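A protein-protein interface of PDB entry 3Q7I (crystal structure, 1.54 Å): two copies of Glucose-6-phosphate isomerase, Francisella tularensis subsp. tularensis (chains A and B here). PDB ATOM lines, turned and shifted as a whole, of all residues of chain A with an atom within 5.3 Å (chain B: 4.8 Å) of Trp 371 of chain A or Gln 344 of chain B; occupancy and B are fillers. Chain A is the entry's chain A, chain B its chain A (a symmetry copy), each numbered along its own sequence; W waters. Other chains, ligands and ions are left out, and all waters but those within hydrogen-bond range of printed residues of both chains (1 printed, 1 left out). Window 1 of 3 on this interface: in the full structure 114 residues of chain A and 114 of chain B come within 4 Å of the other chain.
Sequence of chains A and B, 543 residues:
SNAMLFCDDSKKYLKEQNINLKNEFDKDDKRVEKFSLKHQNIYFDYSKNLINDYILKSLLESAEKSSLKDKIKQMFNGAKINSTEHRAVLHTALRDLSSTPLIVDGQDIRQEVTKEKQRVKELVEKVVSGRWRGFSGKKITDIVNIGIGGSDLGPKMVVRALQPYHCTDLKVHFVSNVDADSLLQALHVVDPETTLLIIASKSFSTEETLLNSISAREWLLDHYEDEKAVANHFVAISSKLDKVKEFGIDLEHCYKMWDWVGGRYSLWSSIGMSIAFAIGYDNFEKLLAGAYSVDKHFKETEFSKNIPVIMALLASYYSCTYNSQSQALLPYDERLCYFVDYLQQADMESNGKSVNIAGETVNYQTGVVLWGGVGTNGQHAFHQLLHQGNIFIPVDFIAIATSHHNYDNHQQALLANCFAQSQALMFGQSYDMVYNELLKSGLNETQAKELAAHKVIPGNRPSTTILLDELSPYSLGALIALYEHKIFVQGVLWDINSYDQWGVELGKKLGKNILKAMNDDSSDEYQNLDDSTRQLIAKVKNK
Water W1 lies within hydrogen-bond range of the backbone carbonyl oxygen of Gly 372 of chain A (2.8 Å) and the side-chain amide nitrogen of Gln 344 of chain B (3.2 Å).
Gln 344 of chain A touches Trp 371 of chain B, and with the chains exchanged Trp 371 of chain A touches Gln 344 of chain B.
Val 369 of chain A touches Trp 371 of chain B, and with the chains exchanged Trp 371 of chain A touches Val 369 of chain B.
5 positions are printed for both chains.
Among the printed residues, pairs that only touch across the chains: Ser 326 of chain A with Val 369 of chain B (3.8 Å), Gln 344 of chain A with Trp 371 of chain B (3.8 Å), Val 369 of chain A with Trp 371 of chain B (3.6 Å), Trp 371 of chain A with Gln 344 of chain B (3.8 Å), Trp 371 of chain A with Met 348 of chain B (3.5 Å), Trp 371 of chain A with Val 369 of chain B (3.6 Å), Gly 372 of chain A with Gln 344 of chain B (3.98 Å), Phe 382 of chain A with Gln 344 of chain B (3.5 Å), Phe 382 of chain A with Met 348 of chain B (3.99 Å) and Ile 393 of chain A with Val 369 of chain B (3.8 Å).
Of the 14 printed residues of chain A, 7 touch a printed residue of chain B.
Hydrophobic or aromatic side chains of chain A within 4 Å of the printed part of chain B: Val 369, Trp 371, Phe 382 and Ile 393.
Among the printed residues, 10 pairs touch across the chains.
NE2 of Gln 344 of chain B lies within hydrogen-bond range of O of Leu 370 of chain B (2.9 Å).
The backbone carbonyl oxygen of Gln 327 of chain A lies within hydrogen-bond range of the backbone NH of Trp 371 of chain A, at 3.1 Å.
The side-chain amide nitrogen (NE2) of Gln 344 of chain A sits at hydrogen-bond distance from the backbone carbonyl oxygen (O) of Leu 370 of chain A (2.9 Å).
O of Trp 371 of chain A is in hydrogen-bond range of N of Leu 329 of chain A.
The side-chain hydroxyl (OG) of Ser 326 of chain A lies within hydrogen-bond range of the indole nitrogen (NE1) of Trp 371 of chain A.
The backbone NH of Gln 327 of chain A sits at hydrogen-bond distance from the backbone carbonyl oxygen of Val 369 of chain A (2.8 Å).
Leu 329 of chain A touches none of the printed residues of chain B.
Of the printed residues of chain B, Trp 371 of chain A touches Gln 344, Met 348 and Val 369.
Printed residues of chain B within 4 Å of Ile 393 of chain A: Val 369 (3.8 Å).
Of the printed residues of chain A, Gln 344 of chain B touches Trp 371, Gly 372 and Phe 382.
Gln 345 of chain B touches none of the printed residues of chain A.
Of the printed residues of chain A, Val 369 of chain B touches Ser 326 (3.8 Å), Trp 371 (3.6 Å) and Ile 393 (3.8 Å).
Of the printed residues of chain A, Trp 371 of chain B touches Gln 344 and Val 369.
The nearest printed residue of chain B that does not touch Trp 371 of chain A is Trp 371 of chain B (4.2 Å).
The nearest printed residue of chain A that does not touch Val 369 of chain B is Val 369 of chain A (5.4 Å).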
ATOM      1  N   SER A 326       2.144  17.822 -34.405  1.00  0.00           N
ATOM      2  CA  SER A 326       2.529  16.690 -33.583  1.00  0.00           C
ATOM      3  C   SER A 326       1.345  16.017 -32.976  1.00  0.00           C
ATOM      4  O   SER A 326       0.220  16.569 -32.963  1.00  0.00           O
ATOM      5  CB  SER A 326       3.497  17.142 -32.444  1.00  0.00           C
ATOM      6  OG  SER A 326       2.808  17.706 -31.355  1.00  0.00           O
ATOM      7  N   GLN A 327       1.565  14.788 -32.523  1.00  0.00           N
ATOM      8  CA  GLN A 327       0.575  14.023 -31.776  1.00  0.00           C
ATOM      9  C   GLN A 327       1.279  13.397 -30.598  1.00  0.00           C
ATOM     10  O   GLN A 327       2.444  12.952 -30.730  1.00  0.00           O
ATOM     11  CB  GLN A 327       0.024  12.878 -32.611  1.00  0.00           C
ATOM     12  CG  GLN A 327      -0.904  13.227 -33.704  1.00  0.00           C
ATOM     13  CD  GLN A 327      -1.234  11.982 -34.546  1.00  0.00           C
ATOM     14  OE1 GLN A 327      -2.252  11.322 -34.320  1.00  0.00           O
ATOM     15  NE2 GLN A 327      -0.315  11.600 -35.482  1.00  0.00           N
ATOM     16  N   ALA A 328       0.605  13.325 -29.438  1.00  0.00           N
ATOM     17  CA  ALA A 328       1.162  12.739 -28.220  1.00  0.00           C
ATOM     18  C   ALA A 328       0.527  11.386 -27.949  1.00  0.00           C
ATOM     19  O   ALA A 328      -0.692  11.223 -28.069  1.00  0.00           O
ATOM     20  CB  ALA A 328       0.918  13.684 -27.052  1.00  0.00           C
ATOM     21  N   LEU A 329       1.359  10.409 -27.563  1.00  0.00           N
ATOM     22  CA  LEU A 329       0.973   9.045 -27.264  1.00  0.00           C
ATOM     23  C   LEU A 329       1.484   8.757 -25.848  1.00  0.00           C
ATOM     24  O   LEU A 329       2.677   8.896 -25.581  1.00  0.00           O
ATOM     25  CB  LEU A 329       1.632   8.109 -28.277  1.00  0.00           C
ATOM     26  CG  LEU A 329       1.433   6.637 -28.012  1.00  0.00           C
ATOM     27  CD1 LEU A 329      -0.031   6.216 -28.019  1.00  0.00           C
ATOM     28  CD2 LEU A 329       2.214   5.883 -29.083  1.00  0.00           C
ATOM     29  N   VAL A 340       6.302   4.251 -27.657  1.00  0.00           N
ATOM     30  CA  VAL A 340       6.415   5.517 -28.400  1.00  0.00           C
ATOM     31  C   VAL A 340       7.570   5.504 -29.409  1.00  0.00           C
ATOM     32  O   VAL A 340       7.390   5.829 -30.560  1.00  0.00           O
ATOM     33  CB  VAL A 340       6.518   6.725 -27.468  1.00  0.00           C
ATOM     34  CG1 VAL A 340       6.843   8.003 -28.248  1.00  0.00           C
ATOM     35  CG2 VAL A 340       5.221   6.866 -26.599  1.00  0.00           C
ATOM     36  N   GLN A 344       7.017   5.930 -33.286  1.00  0.00           N
ATOM     37  CA  GLN A 344       7.656   7.041 -33.903  1.00  0.00           C
ATOM     38  C   GLN A 344       8.343   6.637 -35.214  1.00  0.00           C
ATOM     39  O   GLN A 344       8.186   7.272 -36.246  1.00  0.00           O
ATOM     40  CB  GLN A 344       8.583   7.629 -32.929  1.00  0.00           C
ATOM     41  CG  GLN A 344       9.141   8.881 -33.332  1.00  0.00           C
ATOM     42  CD  GLN A 344      10.082   9.329 -32.276  1.00  0.00           C
ATOM     43  OE1 GLN A 344      11.109   8.683 -32.065  1.00  0.00           O
ATOM     44  NE2 GLN A 344       9.720  10.382 -31.527  1.00  0.00           N
ATOM     45  N   VAL A 369       4.911  14.911 -36.322  1.00  0.00           N
ATOM     46  CA  VAL A 369       5.779  14.341 -35.331  1.00  0.00           C
ATOM     47  C   VAL A 369       4.979  13.527 -34.322  1.00  0.00           C
ATOM     48  O   VAL A 369       3.956  14.000 -33.788  1.00  0.00           O
ATOM     49  CB  VAL A 369       6.535  15.438 -34.577  1.00  0.00           C
ATOM     50  CG1 VAL A 369       7.382  14.872 -33.375  1.00  0.00           C
ATOM     51  CG2 VAL A 369       7.465  16.217 -35.556  1.00  0.00           C
ATOM     52  N   LEU A 370       5.419  12.333 -34.012  1.00  0.00           N
ATOM     53  CA  LEU A 370       4.824  11.519 -32.960  1.00  0.00           C
ATOM     54  C   LEU A 370       5.787  11.537 -31.783  1.00  0.00           C
ATOM     55  O   LEU A 370       6.990  11.306 -31.949  1.00  0.00           O
ATOM     56  CB  LEU A 370       4.614  10.063 -33.368  1.00  0.00           C
ATOM     57  CG  LEU A 370       3.838   9.145 -32.428  1.00  0.00           C
ATOM     58  CD1 LEU A 370       2.407   9.618 -32.156  1.00  0.00           C
ATOM     59  CD2 LEU A 370       3.812   7.705 -32.957  1.00  0.00           C
ATOM     60  N   TRP A 371       5.264  11.777 -30.590  1.00  0.00           N
ATOM     61  CA  TRP A 371       6.048  11.831 -29.370  1.00  0.00           C
ATOM     62  C   TRP A 371       5.196  11.418 -28.198  1.00  0.00           C
ATOM     63  O   TRP A 371       3.970  11.185 -28.342  1.00  0.00           O
ATOM     64  CB  TRP A 371       6.648  13.234 -29.195  1.00  0.00           C
ATOM     65  CG  TRP A 371       5.622  14.291 -28.946  1.00  0.00           C
ATOM     66  CD1 TRP A 371       4.799  14.897 -29.858  1.00  0.00           C
ATOM     67  CD2 TRP A 371       5.217  14.804 -27.655  1.00  0.00           C
ATOM     68  NE1 TRP A 371       3.925  15.734 -29.238  1.00  0.00           N
ATOM     69  CE2 TRP A 371       4.175  15.723 -27.880  1.00  0.00           C
ATOM     70  CE3 TRP A 371       5.695  14.625 -26.352  1.00  0.00           C
ATOM     71  CZ2 TRP A 371       3.551  16.421 -26.862  1.00  0.00           C
ATOM     72  CZ3 TRP A 371       5.057  15.320 -25.330  1.00  0.00           C
ATOM     73  CH2 TRP A 371       4.006  16.195 -25.566  1.00  0.00           C
ATOM     74  N   GLY A 372       5.791  11.398 -27.017  1.00  0.00           N
ATOM     75  CA  GLY A 372       4.986  11.135 -25.838  1.00  0.00           C
ATOM     76  C   GLY A 372       5.839  10.618 -24.703  1.00  0.00           C
ATOM     77  O   GLY A 372       6.978  11.037 -24.532  1.00  0.00           O
ATOM     78  N   GLY A 373       5.219   9.825 -23.847  1.00  0.00           N
ATOM     79  CA  GLY A 373       5.911   9.303 -22.714  1.00  0.00           C
ATOM     80  C   GLY A 373       4.990   8.552 -21.759  1.00  0.00           C
ATOM     81  O   GLY A 373       3.759   8.724 -21.814  1.00  0.00           O
ATOM     82  N   PHE A 382       5.908  16.859 -19.128  1.00  0.00           N
ATOM     83  CA  PHE A 382       5.362  17.543 -20.251  1.00  0.00           C
ATOM     84  C   PHE A 382       3.862  17.682 -20.241  1.00  0.00           C
ATOM     85  O   PHE A 382       3.309  18.434 -21.062  1.00  0.00           O
ATOM     86  CB  PHE A 382       5.871  16.871 -21.514  1.00  0.00           C
ATOM     87  CG  PHE A 382       5.513  15.427 -21.596  1.00  0.00           C
ATOM     88  CD1 PHE A 382       4.235  15.032 -21.948  1.00  0.00           C
ATOM     89  CD2 PHE A 382       6.444  14.468 -21.260  1.00  0.00           C
ATOM     90  CE1 PHE A 382       3.901  13.712 -22.024  1.00  0.00           C
ATOM     91  CE2 PHE A 382       6.091  13.117 -21.266  1.00  0.00           C
ATOM     92  CZ  PHE A 382       4.799  12.748 -21.672  1.00  0.00           C
ATOM     93  N   LEU A 386       0.701  20.095 -22.207  1.00  0.00           N
ATOM     94  CA  LEU A 386      -0.614  19.621 -22.682  1.00  0.00           C
ATOM     95  C   LEU A 386      -1.765  20.343 -22.037  1.00  0.00           C
ATOM     96  O   LEU A 386      -2.773  20.565 -22.707  1.00  0.00           O
ATOM     97  CB  LEU A 386      -0.756  18.093 -22.466  1.00  0.00           C
ATOM     98  CG  LEU A 386       0.268  17.200 -23.175  1.00  0.00           C
ATOM     99  CD1 LEU A 386      -0.052  15.703 -22.794  1.00  0.00           C
ATOM    100  CD2 LEU A 386       0.286  17.417 -24.710  1.00  0.00           C
ATOM    101  N   ILE A 393      -2.433  19.805 -29.744  1.00  0.00           N
ATOM    102  CA  ILE A 393      -1.810  18.478 -29.785  1.00  0.00           C
ATOM    103  C   ILE A 393      -2.892  17.425 -29.501  1.00  0.00           C
ATOM    104  O   ILE A 393      -3.322  17.278 -28.342  1.00  0.00           O
ATOM    105  CB  ILE A 393      -0.665  18.356 -28.751  1.00  0.00           C
ATOM    106  CG1 ILE A 393       0.334  19.484 -28.934  1.00  0.00           C
ATOM    107  CG2 ILE A 393       0.001  16.947 -28.860  1.00  0.00           C
ATOM    108  CD1 ILE A 393       1.329  19.639 -27.760  1.00  0.00           C
ATOM    109  N   VAL B 340      17.151  13.394 -24.035  1.00  0.00           N
ATOM    110  CA  VAL B 340      15.914  13.973 -24.583  1.00  0.00           C
ATOM    111  C   VAL B 340      14.765  13.975 -23.566  1.00  0.00           C
ATOM    112  O   VAL B 340      14.134  14.983 -23.347  1.00  0.00           O
ATOM    113  CB  VAL B 340      15.488  13.295 -25.885  1.00  0.00           C
ATOM    114  CG1 VAL B 340      14.098  13.766 -26.328  1.00  0.00           C
ATOM    115  CG2 VAL B 340      16.574  13.502 -26.997  1.00  0.00           C
ATOM    116  N   ASP B 341      14.523  12.831 -22.887  1.00  0.00           N
ATOM    117  CA  ASP B 341      13.444  12.763 -21.911  1.00  0.00           C
ATOM    118  C   ASP B 341      13.619  13.842 -20.833  1.00  0.00           C
ATOM    119  O   ASP B 341      12.646  14.491 -20.405  1.00  0.00           O
ATOM    120  CB  ASP B 341      13.427  11.406 -21.263  1.00  0.00           C
ATOM    121  CG  ASP B 341      12.850  10.334 -22.150  1.00  0.00           C
ATOM    122  OD1 ASP B 341      12.258  10.683 -23.176  1.00  0.00           O
ATOM    123  OD2 ASP B 341      12.976   9.162 -21.747  1.00  0.00           O
ATOM    124  N   TYR B 342      14.849  13.985 -20.344  1.00  0.00           N
ATOM    125  CA  TYR B 342      15.191  14.948 -19.316  1.00  0.00           C
ATOM    126  C   TYR B 342      14.903  16.355 -19.746  1.00  0.00           C
ATOM    127  O   TYR B 342      14.289  17.125 -19.024  1.00  0.00           O
ATOM    128  CB  TYR B 342      16.660  14.762 -18.869  1.00  0.00           C
ATOM    129  CG  TYR B 342      16.986  15.777 -17.795  1.00  0.00           C
ATOM    130  CD1 TYR B 342      16.609  15.567 -16.457  1.00  0.00           C
ATOM    131  CD2 TYR B 342      17.612  16.954 -18.118  1.00  0.00           C
ATOM    132  CE1 TYR B 342      16.891  16.529 -15.486  1.00  0.00           C
ATOM    133  CE2 TYR B 342      17.899  17.920 -17.145  1.00  0.00           C
ATOM    134  CZ  TYR B 342      17.526  17.680 -15.860  1.00  0.00           C
ATOM    135  OH  TYR B 342      17.778  18.575 -14.841  1.00  0.00           O
ATOM    136  N   LEU B 343      15.375  16.711 -20.917  1.00  0.00           N
ATOM    137  CA  LEU B 343      15.202  18.089 -21.463  1.00  0.00           C
ATOM    138  C   LEU B 343      13.760  18.301 -21.873  1.00  0.00           C
ATOM    139  O   LEU B 343      13.273  19.458 -21.821  1.00  0.00           O
ATOM    140  CB  LEU B 343      16.209  18.452 -22.516  1.00  0.00           C
ATOM    141  CG  LEU B 343      17.613  18.613 -21.979  1.00  0.00           C
ATOM    142  CD1 LEU B 343      18.482  19.016 -23.141  1.00  0.00           C
ATOM    143  CD2 LEU B 343      17.825  19.596 -20.840  1.00  0.00           C
ATOM    144  N   GLN B 344      13.043  17.284 -22.302  1.00  0.00           N
ATOM    145  CA  GLN B 344      11.649  17.414 -22.552  1.00  0.00           C
ATOM    146  C   GLN B 344      10.900  17.919 -21.313  1.00  0.00           C
ATOM    147  O   GLN B 344      10.106  18.845 -21.373  1.00  0.00           O
ATOM    148  CB  GLN B 344      11.153  16.118 -23.031  1.00  0.00           C
ATOM    149  CG  GLN B 344       9.812  16.151 -23.527  1.00  0.00           C
ATOM    150  CD  GLN B 344       9.438  14.773 -23.933  1.00  0.00           C
ATOM    151  OE1 GLN B 344       9.340  13.894 -23.076  1.00  0.00           O
ATOM    152  NE2 GLN B 344       9.309  14.526 -25.246  1.00  0.00           N
ATOM    153  N   GLN B 345      11.197  17.366 -20.133  1.00  0.00           N
ATOM    154  CA  GLN B 345      10.676  17.902 -18.940  1.00  0.00           C
ATOM    155  C   GLN B 345      11.155  19.328 -18.676  1.00  0.00           C
ATOM    156  O   GLN B 345      10.324  20.223 -18.418  1.00  0.00           O
ATOM    157  CB  GLN B 345      11.055  16.975 -17.766  1.00  0.00           C
ATOM    158  CG  GLN B 345      10.638  17.539 -16.441  1.00  0.00           C
ATOM    159  CD  GLN B 345      10.675  16.570 -15.249  1.00  0.00           C
ATOM    160  OE1 GLN B 345      11.126  15.426 -15.341  1.00  0.00           O
ATOM    161  NE2 GLN B 345      10.175  17.060 -14.133  1.00  0.00           N
ATOM    162  N   ALA B 346      12.477  19.522 -18.678  1.00  0.00           N
ATOM    163  CA  ALA B 346      12.981  20.869 -18.329  1.00  0.00           C
ATOM    164  C   ALA B 346      12.378  21.943 -19.201  1.00  0.00           C
ATOM    165  O   ALA B 346      12.015  23.030 -18.715  1.00  0.00           O
ATOM    166  CB  ALA B 346      14.485  20.945 -18.436  1.00  0.00           C
ATOM    167  N   ASP B 347      12.299  21.680 -20.496  1.00  0.00           N
ATOM    168  CA  ASP B 347      11.830  22.681 -21.478  1.00  0.00           C
ATOM    169  C   ASP B 347      10.315  22.794 -21.421  1.00  0.00           C
ATOM    170  O   ASP B 347       9.786  23.871 -21.119  1.00  0.00           O
ATOM    171  CB  ASP B 347      12.338  22.255 -22.850  1.00  0.00           C
ATOM    172  CG  ASP B 347      12.091  23.225 -23.918  1.00  0.00           C
ATOM    173  OD1 ASP B 347      11.373  24.194 -23.719  1.00  0.00           O
ATOM    174  OD2 ASP B 347      12.666  23.022 -25.003  1.00  0.00           O
ATOM    175  N   MET B 348       9.594  21.720 -21.732  1.00  0.00           N
ATOM    176  CA  MET B 348       8.123  21.837 -21.910  1.00  0.00           C
ATOM    177  C   MET B 348       7.413  22.188 -20.624  1.00  0.00           C
ATOM    178  O   MET B 348       6.389  22.890 -20.649  1.00  0.00           O
ATOM    179  CB  MET B 348       7.569  20.526 -22.480  1.00  0.00           C
ATOM    180  CG  MET B 348       8.140  20.253 -23.843  1.00  0.00           C
ATOM    181  SD  MET B 348       7.532  18.734 -24.623  1.00  0.00           S
ATOM    182  CE  MET B 348       5.952  19.002 -24.886  1.00  0.00           C
ATOM    183  N   GLU B 349       7.859  21.642 -19.501  1.00  0.00           N
ATOM    184  CA  GLU B 349       7.209  21.992 -18.239  1.00  0.00           C
ATOM    185  C   GLU B 349       7.514  23.456 -17.858  1.00  0.00           C
ATOM    186  O   GLU B 349       6.694  24.103 -17.200  1.00  0.00           O
ATOM    187  CB  GLU B 349       7.636  21.059 -17.106  1.00  0.00           C
ATOM    188  CG  GLU B 349       6.720  21.160 -15.935  1.00  0.00           C
ATOM    189  CD  GLU B 349       7.162  20.323 -14.763  1.00  0.00           C
ATOM    190  OE1 GLU B 349       8.264  19.726 -14.808  1.00  0.00           O
ATOM    191  OE2 GLU B 349       6.472  20.421 -13.742  1.00  0.00           O
ATOM    192  N   VAL B 369       7.037  21.621 -28.582  1.00  0.00           N
ATOM    193  CA  VAL B 369       7.343  20.265 -28.225  1.00  0.00           C
ATOM    194  C   VAL B 369       8.820  19.968 -28.458  1.00  0.00           C
ATOM    195  O   VAL B 369       9.368  20.272 -29.535  1.00  0.00           O
ATOM    196  CB  VAL B 369       6.515  19.284 -29.062  1.00  0.00           C
ATOM    197  CG1 VAL B 369       6.927  17.784 -28.817  1.00  0.00           C
ATOM    198  CG2 VAL B 369       4.998  19.471 -28.757  1.00  0.00           C
ATOM    199  N   LEU B 370       9.479  19.358 -27.505  1.00  0.00           N
ATOM    200  CA  LEU B 370      10.851  18.895 -27.664  1.00  0.00           C
ATOM    201  C   LEU B 370      10.799  17.381 -27.795  1.00  0.00           C
ATOM    202  O   LEU B 370      10.152  16.700 -26.991  1.00  0.00           O
ATOM    203  CB  LEU B 370      11.743  19.229 -26.473  1.00  0.00           C
ATOM    204  CG  LEU B 370      13.242  18.962 -26.583  1.00  0.00           C
ATOM    205  CD1 LEU B 370      13.917  19.731 -27.722  1.00  0.00           C
ATOM    206  CD2 LEU B 370      13.959  19.270 -25.261  1.00  0.00           C
ATOM    207  N   TRP B 371      11.503  16.844 -28.779  1.00  0.00           N
ATOM    208  CA  TRP B 371      11.556  15.417 -29.040  1.00  0.00           C
ATOM    209  C   TRP B 371      12.875  15.062 -29.674  1.00  0.00           C
ATOM    210  O   TRP B 371      13.699  15.957 -29.993  1.00  0.00           O
ATOM    211  CB  TRP B 371      10.356  14.997 -29.903  1.00  0.00           C
ATOM    212  CG  TRP B 371      10.395  15.562 -31.285  1.00  0.00           C
ATOM    213  CD1 TRP B 371      10.075  16.832 -31.686  1.00  0.00           C
ATOM    214  CD2 TRP B 371      10.894  14.894 -32.468  1.00  0.00           C
ATOM    215  NE1 TRP B 371      10.336  17.000 -33.010  1.00  0.00           N
ATOM    216  CE2 TRP B 371      10.815  15.815 -33.531  1.00  0.00           C
ATOM    217  CE3 TRP B 371      11.321  13.588 -32.733  1.00  0.00           C
ATOM    218  CZ2 TRP B 371      11.200  15.511 -34.824  1.00  0.00           C
ATOM    219  CZ3 TRP B 371      11.717  13.289 -34.033  1.00  0.00           C
ATOM    220  CH2 TRP B 371      11.668  14.221 -35.060  1.00  0.00           C
HETATM  221  O   HOH W   1       8.706  11.736 -26.623  1.00  0.00           O
